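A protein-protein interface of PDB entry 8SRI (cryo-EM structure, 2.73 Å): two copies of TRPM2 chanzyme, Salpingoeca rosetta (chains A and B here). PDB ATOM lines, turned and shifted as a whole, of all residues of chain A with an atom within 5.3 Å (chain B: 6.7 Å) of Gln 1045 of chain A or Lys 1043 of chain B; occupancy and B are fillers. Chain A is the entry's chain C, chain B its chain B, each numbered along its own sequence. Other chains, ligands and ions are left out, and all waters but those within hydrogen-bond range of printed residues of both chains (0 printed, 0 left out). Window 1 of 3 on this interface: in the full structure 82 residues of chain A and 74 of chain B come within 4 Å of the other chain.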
ATOM      1  N   MET A 930     -27.373  12.686 -24.852  1.00  0.00           N
ATOM      2  CA  MET A 930     -26.311  12.104 -25.692  1.00  0.00           C
ATOM      3  C   MET A 930     -26.866  11.086 -26.679  1.00  0.00           C
ATOM      4  O   MET A 930     -26.420  11.068 -27.822  1.00  0.00           O
ATOM      5  CB  MET A 930     -25.205  11.458 -24.859  1.00  0.00           C
ATOM      6  CG  MET A 930     -24.393  12.408 -24.035  1.00  0.00           C
ATOM      7  SD  MET A 930     -23.453  11.498 -22.817  1.00  0.00           S
ATOM      8  CE  MET A 930     -23.106  12.817 -21.676  1.00  0.00           C
ATOM      9  N   THR A1040     -18.200  11.312 -30.982  1.00  0.00           N
ATOM     10  CA  THR A1040     -19.421  12.086 -30.754  1.00  0.00           C
ATOM     11  C   THR A1040     -19.652  12.321 -29.260  1.00  0.00           C
ATOM     12  O   THR A1040     -19.948  13.463 -28.873  1.00  0.00           O
ATOM     13  CB  THR A1040     -20.600  11.351 -31.416  1.00  0.00           C
ATOM     14  OG1 THR A1040     -20.370  11.283 -32.828  1.00  0.00           O
ATOM     15  CG2 THR A1040     -21.931  12.085 -31.223  1.00  0.00           C
ATOM     16  N   TYR A1041     -19.415  11.262 -28.433  1.00  0.00           N
ATOM     17  CA  TYR A1041     -19.520  11.258 -26.961  1.00  0.00           C
ATOM     18  C   TYR A1041     -18.572  12.284 -26.333  1.00  0.00           C
ATOM     19  O   TYR A1041     -19.001  13.094 -25.484  1.00  0.00           O
ATOM     20  CB  TYR A1041     -19.227   9.838 -26.443  1.00  0.00           C
ATOM     21  CG  TYR A1041     -19.620   9.540 -25.004  1.00  0.00           C
ATOM     22  CD1 TYR A1041     -18.716   9.778 -23.943  1.00  0.00           C
ATOM     23  CD2 TYR A1041     -20.880   8.972 -24.708  1.00  0.00           C
ATOM     24  CE1 TYR A1041     -19.065   9.512 -22.635  1.00  0.00           C
ATOM     25  CE2 TYR A1041     -21.235   8.678 -23.375  1.00  0.00           C
ATOM     26  CZ  TYR A1041     -20.305   8.962 -22.362  1.00  0.00           C
ATOM     27  OH  TYR A1041     -20.574   8.723 -21.045  1.00  0.00           O
ATOM     28  N   MET A1042     -17.268  12.217 -26.728  1.00  0.00           N
ATOM     29  CA  MET A1042     -16.230  13.167 -26.284  1.00  0.00           C
ATOM     30  C   MET A1042     -16.538  14.607 -26.718  1.00  0.00           C
ATOM     31  O   MET A1042     -16.148  15.554 -26.023  1.00  0.00           O
ATOM     32  CB  MET A1042     -14.838  12.752 -26.765  1.00  0.00           C
ATOM     33  CG  MET A1042     -14.312  11.472 -26.144  1.00  0.00           C
ATOM     34  SD  MET A1042     -14.074  11.610 -24.364  1.00  0.00           S
ATOM     35  CE  MET A1042     -13.311  10.030 -24.013  1.00  0.00           C
ATOM     36  N   LYS A1043     -17.195  14.782 -27.881  1.00  0.00           N
ATOM     37  CA  LYS A1043     -17.507  16.119 -28.379  1.00  0.00           C
ATOM     38  C   LYS A1043     -18.657  16.754 -27.593  1.00  0.00           C
ATOM     39  O   LYS A1043     -18.597  17.948 -27.276  1.00  0.00           O
ATOM     40  CB  LYS A1043     -17.836  16.094 -29.871  1.00  0.00           C
ATOM     41  CG  LYS A1043     -16.618  16.108 -30.772  1.00  0.00           C
ATOM     42  CD  LYS A1043     -17.007  15.963 -32.234  1.00  0.00           C
ATOM     43  CE  LYS A1043     -15.838  16.248 -33.173  1.00  0.00           C
ATOM     44  NZ  LYS A1043     -14.495  16.222 -32.519  1.00  0.00           N
ATOM     45  N   VAL A1044     -19.707  15.988 -27.245  1.00  0.00           N
ATOM     46  CA  VAL A1044     -20.943  16.636 -26.800  1.00  0.00           C
ATOM     47  C   VAL A1044     -21.301  16.321 -25.339  1.00  0.00           C
ATOM     48  O   VAL A1044     -22.413  16.670 -24.908  1.00  0.00           O
ATOM     49  CB  VAL A1044     -22.152  16.349 -27.736  1.00  0.00           C
ATOM     50  CG1 VAL A1044     -21.902  16.815 -29.181  1.00  0.00           C
ATOM     51  CG2 VAL A1044     -22.737  14.878 -27.699  1.00  0.00           C
ATOM     52  N   GLN A1045     -20.357  15.733 -24.547  1.00  0.00           N
ATOM     53  CA  GLN A1045     -20.570  15.452 -23.108  1.00  0.00           C
ATOM     54  C   GLN A1045     -20.796  16.704 -22.231  1.00  0.00           C
ATOM     55  O   GLN A1045     -21.742  16.728 -21.422  1.00  0.00           O
ATOM     56  CB  GLN A1045     -19.344  14.693 -22.582  1.00  0.00           C
ATOM     57  CG  GLN A1045     -19.521  13.923 -21.282  1.00  0.00           C
ATOM     58  CD  GLN A1045     -18.263  13.193 -20.847  1.00  0.00           C
ATOM     59  OE1 GLN A1045     -17.272  13.153 -21.575  1.00  0.00           O
ATOM     60  NE2 GLN A1045     -18.299  12.615 -19.651  1.00  0.00           N
ATOM     61  N   GLU A1046     -19.987  17.762 -22.434  1.00  0.00           N
ATOM     62  CA  GLU A1046     -20.109  19.014 -21.674  1.00  0.00           C
ATOM     63  C   GLU A1046     -21.367  19.796 -22.059  1.00  0.00           C
ATOM     64  O   GLU A1046     -22.032  20.399 -21.197  1.00  0.00           O
ATOM     65  CB  GLU A1046     -18.860  19.870 -21.882  1.00  0.00           C
ATOM     66  CG  GLU A1046     -17.573  19.228 -21.384  1.00  0.00           C
ATOM     67  CD  GLU A1046     -17.336  19.464 -19.905  1.00  0.00           C
ATOM     68  OE1 GLU A1046     -17.713  20.545 -19.404  1.00  0.00           O
ATOM     69  OE2 GLU A1046     -16.765  18.572 -19.244  1.00  0.00           O
ATOM     70  N   ALA A1047     -21.676  19.790 -23.367  1.00  0.00           N
ATOM     71  CA  ALA A1047     -22.895  20.376 -23.923  1.00  0.00           C
ATOM     72  C   ALA A1047     -24.149  19.665 -23.431  1.00  0.00           C
ATOM     73  O   ALA A1047     -25.192  20.307 -23.254  1.00  0.00           O
ATOM     74  CB  ALA A1047     -22.833  20.355 -25.449  1.00  0.00           C
ATOM     75  N   ALA A1048     -24.072  18.327 -23.283  1.00  0.00           N
ATOM     76  CA  ALA A1048     -25.157  17.526 -22.716  1.00  0.00           C
ATOM     77  C   ALA A1048     -25.421  17.875 -21.256  1.00  0.00           C
ATOM     78  O   ALA A1048     -26.585  17.880 -20.832  1.00  0.00           O
ATOM     79  CB  ALA A1048     -24.837  16.039 -22.863  1.00  0.00           C
ATOM     80  N   GLU A1049     -24.344  18.104 -20.470  1.00  0.00           N
ATOM     81  CA  GLU A1049     -24.478  18.559 -19.075  1.00  0.00           C
ATOM     82  C   GLU A1049     -25.123  19.948 -18.967  1.00  0.00           C
ATOM     83  O   GLU A1049     -25.983  20.173 -18.092  1.00  0.00           O
ATOM     84  CB  GLU A1049     -23.123  18.553 -18.365  1.00  0.00           C
ATOM     85  CG  GLU A1049     -22.513  17.180 -18.171  1.00  0.00           C
ATOM     86  CD  GLU A1049     -22.964  16.532 -16.879  1.00  0.00           C
ATOM     87  OE1 GLU A1049     -23.455  17.260 -15.990  1.00  0.00           O
ATOM     88  OE2 GLU A1049     -22.828  15.297 -16.749  1.00  0.00           O
ATOM     89  N   ASN B1038     -15.184   3.460 -22.286  1.00  0.00           N
ATOM     90  CA  ASN B1038     -13.897   4.088 -22.662  1.00  0.00           C
ATOM     91  C   ASN B1038     -13.636   5.392 -21.906  1.00  0.00           C
ATOM     92  O   ASN B1038     -12.518   5.594 -21.391  1.00  0.00           O
ATOM     93  CB  ASN B1038     -13.790   4.401 -24.166  1.00  0.00           C
ATOM     94  CG  ASN B1038     -13.699   3.175 -25.061  1.00  0.00           C
ATOM     95  OD1 ASN B1038     -14.599   2.870 -25.835  1.00  0.00           O
ATOM     96  ND2 ASN B1038     -12.555   2.521 -25.020  1.00  0.00           N
ATOM     97  N   ASP B1039     -14.683   6.240 -21.787  1.00  0.00           N
ATOM     98  CA  ASP B1039     -14.615   7.511 -21.055  1.00  0.00           C
ATOM     99  C   ASP B1039     -14.401   7.306 -19.556  1.00  0.00           C
ATOM    100  O   ASP B1039     -13.563   7.993 -18.945  1.00  0.00           O
ATOM    101  CB  ASP B1039     -15.872   8.326 -21.306  1.00  0.00           C
ATOM    102  CG  ASP B1039     -15.856   9.656 -20.587  1.00  0.00           C
ATOM    103  OD1 ASP B1039     -14.918  10.446 -20.827  1.00  0.00           O
ATOM    104  OD2 ASP B1039     -16.778   9.914 -19.786  1.00  0.00           O
ATOM    105  N   THR B1040     -15.172   6.361 -18.971  1.00  0.00           N
ATOM    106  CA  THR B1040     -15.137   5.996 -17.554  1.00  0.00           C
ATOM    107  C   THR B1040     -13.774   5.419 -17.167  1.00  0.00           C
ATOM    108  O   THR B1040     -13.222   5.830 -16.135  1.00  0.00           O
ATOM    109  CB  THR B1040     -16.286   5.013 -17.270  1.00  0.00           C
ATOM    110  OG1 THR B1040     -17.533   5.668 -17.535  1.00  0.00           O
ATOM    111  CG2 THR B1040     -16.328   4.566 -15.805  1.00  0.00           C
ATOM    112  N   TYR B1041     -13.207   4.550 -18.053  1.00  0.00           N
ATOM    113  CA  TYR B1041     -11.886   3.905 -17.926  1.00  0.00           C
ATOM    114  C   TYR B1041     -10.766   4.945 -17.843  1.00  0.00           C
ATOM    115  O   TYR B1041      -9.911   4.872 -16.932  1.00  0.00           O
ATOM    116  CB  TYR B1041     -11.677   2.956 -19.118  1.00  0.00           C
ATOM    117  CG  TYR B1041     -10.547   1.945 -18.997  1.00  0.00           C
ATOM    118  CD1 TYR B1041      -9.238   2.268 -19.425  1.00  0.00           C
ATOM    119  CD2 TYR B1041     -10.797   0.645 -18.501  1.00  0.00           C
ATOM    120  CE1 TYR B1041      -8.207   1.357 -19.317  1.00  0.00           C
ATOM    121  CE2 TYR B1041      -9.753  -0.298 -18.409  1.00  0.00           C
ATOM    122  CZ  TYR B1041      -8.469   0.091 -18.824  1.00  0.00           C
ATOM    123  OH  TYR B1041      -7.399  -0.754 -18.753  1.00  0.00           O
ATOM    124  N   MET B1042     -10.750   5.894 -18.823  1.00  0.00           N
ATOM    125  CA  MET B1042      -9.791   7.014 -18.863  1.00  0.00           C
ATOM    126  C   MET B1042      -9.923   7.934 -17.642  1.00  0.00           C
ATOM    127  O   MET B1042      -8.929   8.537 -17.218  1.00  0.00           O
ATOM    128  CB  MET B1042      -9.916   7.823 -20.156  1.00  0.00           C
ATOM    129  CG  MET B1042      -9.506   7.074 -21.410  1.00  0.00           C
ATOM    130  SD  MET B1042      -7.762   6.622 -21.410  1.00  0.00           S
ATOM    131  CE  MET B1042      -7.605   5.932 -23.054  1.00  0.00           C
ATOM    132  N   LYS B1043     -11.146   8.082 -17.100  1.00  0.00           N
ATOM    133  CA  LYS B1043     -11.364   8.957 -15.951  1.00  0.00           C
ATOM    134  C   LYS B1043     -10.831   8.330 -14.661  1.00  0.00           C
ATOM    135  O   LYS B1043     -10.222   9.032 -13.845  1.00  0.00           O
ATOM    136  CB  LYS B1043     -12.842   9.312 -15.795  1.00  0.00           C
ATOM    137  CG  LYS B1043     -13.299  10.456 -16.677  1.00  0.00           C
ATOM    138  CD  LYS B1043     -14.797  10.681 -16.562  1.00  0.00           C
ATOM    139  CE  LYS B1043     -15.236  11.988 -17.219  1.00  0.00           C
ATOM    140  NZ  LYS B1043     -14.236  12.578 -18.160  1.00  0.00           N
ATOM    141  N   VAL B1044     -11.020   7.014 -14.451  1.00  0.00           N
ATOM    142  CA  VAL B1044     -10.822   6.474 -13.105  1.00  0.00           C
ATOM    143  C   VAL B1044      -9.666   5.464 -13.019  1.00  0.00           C
ATOM    144  O   VAL B1044      -9.517   4.813 -11.971  1.00  0.00           O
ATOM    145  CB  VAL B1044     -12.121   5.873 -12.493  1.00  0.00           C
ATOM    146  CG1 VAL B1044     -13.257   6.906 -12.394  1.00  0.00           C
ATOM    147  CG2 VAL B1044     -12.632   4.513 -13.123  1.00  0.00           C
ATOM    148  N   GLN B1045      -8.800   5.374 -14.070  1.00  0.00           N
ATOM    149  CA  GLN B1045      -7.610   4.490 -14.064  1.00  0.00           C
ATOM    150  C   GLN B1045      -6.559   4.827 -12.984  1.00  0.00           C
ATOM    151  O   GLN B1045      -6.094   3.920 -12.269  1.00  0.00           O
ATOM    152  CB  GLN B1045      -6.945   4.572 -15.445  1.00  0.00           C
ATOM    153  CG  GLN B1045      -5.995   3.443 -15.817  1.00  0.00           C
ATOM    154  CD  GLN B1045      -5.398   3.600 -17.203  1.00  0.00           C
ATOM    155  OE1 GLN B1045      -5.778   4.495 -17.958  1.00  0.00           O
ATOM    156  NE2 GLN B1045      -4.454   2.728 -17.542  1.00  0.00           N
ATOM    157  N   GLU B1046      -6.236   6.124 -12.811  1.00  0.00           N
ATOM    158  CA  GLU B1046      -5.260   6.574 -11.809  1.00  0.00           C
ATOM    159  C   GLU B1046      -5.798   6.432 -10.383  1.00  0.00           C
ATOM    160  O   GLU B1046      -5.056   6.065  -9.454  1.00  0.00           O
ATOM    161  CB  GLU B1046      -4.860   8.022 -12.089  1.00  0.00           C
ATOM    162  CG  GLU B1046      -4.172   8.232 -13.431  1.00  0.00           C
ATOM    163  CD  GLU B1046      -2.681   7.962 -13.374  1.00  0.00           C
ATOM    164  OE1 GLU B1046      -2.064   8.236 -12.324  1.00  0.00           O
ATOM    165  OE2 GLU B1046      -2.124   7.482 -14.384  1.00  0.00           O
ATOM    166  N   ALA B1047      -7.096   6.740 -10.220  1.00  0.00           N
ATOM    167  CA  ALA B1047      -7.829   6.561  -8.967  1.00  0.00           C
ATOM    168  C   ALA B1047      -7.935   5.095  -8.570  1.00  0.00           C
ATOM    169  O   ALA B1047      -7.927   4.779  -7.373  1.00  0.00           O
ATOM    170  CB  ALA B1047      -9.219   7.184  -9.084  1.00  0.00           C
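Asp 1039 of chain B touches Tyr 1041 of chain A.
Asp 1039 of chain B touches Met 1042 of chain A (OD1 to CE, 3.6 Å).
NE2 of Gln 1045 of chain A touches CE of Lys 1043 of chain B, 3.96 Å away.
Of the 11 printed residues of chain A, 3 touch a printed residue of chain B.
Of the 10 printed residues of chain B, 2 touch a printed residue of chain A.
Among the printed residues, 4 pairs touch across the chains.
Among the printed residues, no Asp or Glu carboxylate lies within 4 Å of a Lys or Arg side-chain nitrogen of the other chain.
NZ of Lys 1043 of chain B is in salt-bridge range of OD1 of Asp 1039 of chain B.
Gln 1045 of chain A touches Lys 1043 of chain B, but with the chains exchanged Lys 1043 of chain A does not touch Gln 1045 of chain B (18.3 Å).
Positions printed for both chains: 1040, 1041, 1042, 1043, 1044, 1045, 1046 and 1047.
Of the 4 pairs that touch across the chains among the printed residues, none has its exchanged pair printed and touching as well.
OD2 of Asp 1039 of chain B is in hydrogen-bond range of NE2 of Gln 1045 of chain A (3.1 Å).
Printed residues of chain B within 4 Å of Tyr 1041 of chain A: Asp 1039 (3.7 Å).
Printed residues of chain B within 4 Å of Met 1042 of chain A: Asp 1039 (3.6 Å).
Val 1044 of chain A touches none of the printed residues of chain B.
Of chain B, only Asp 1039 (3.1 Å) and Lys 1043 (3.96 Å) come within 4 Å of Gln 1045 of chain A.
Of the printed residues of chain A, Asp 1039 of chain B touches Tyr 1041, Met 1042 and Gln 1045.
The nearest printed residue of chain B that does not touch Met 1042 of chain A is Asn 1038 of chain B (5.1 Å).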
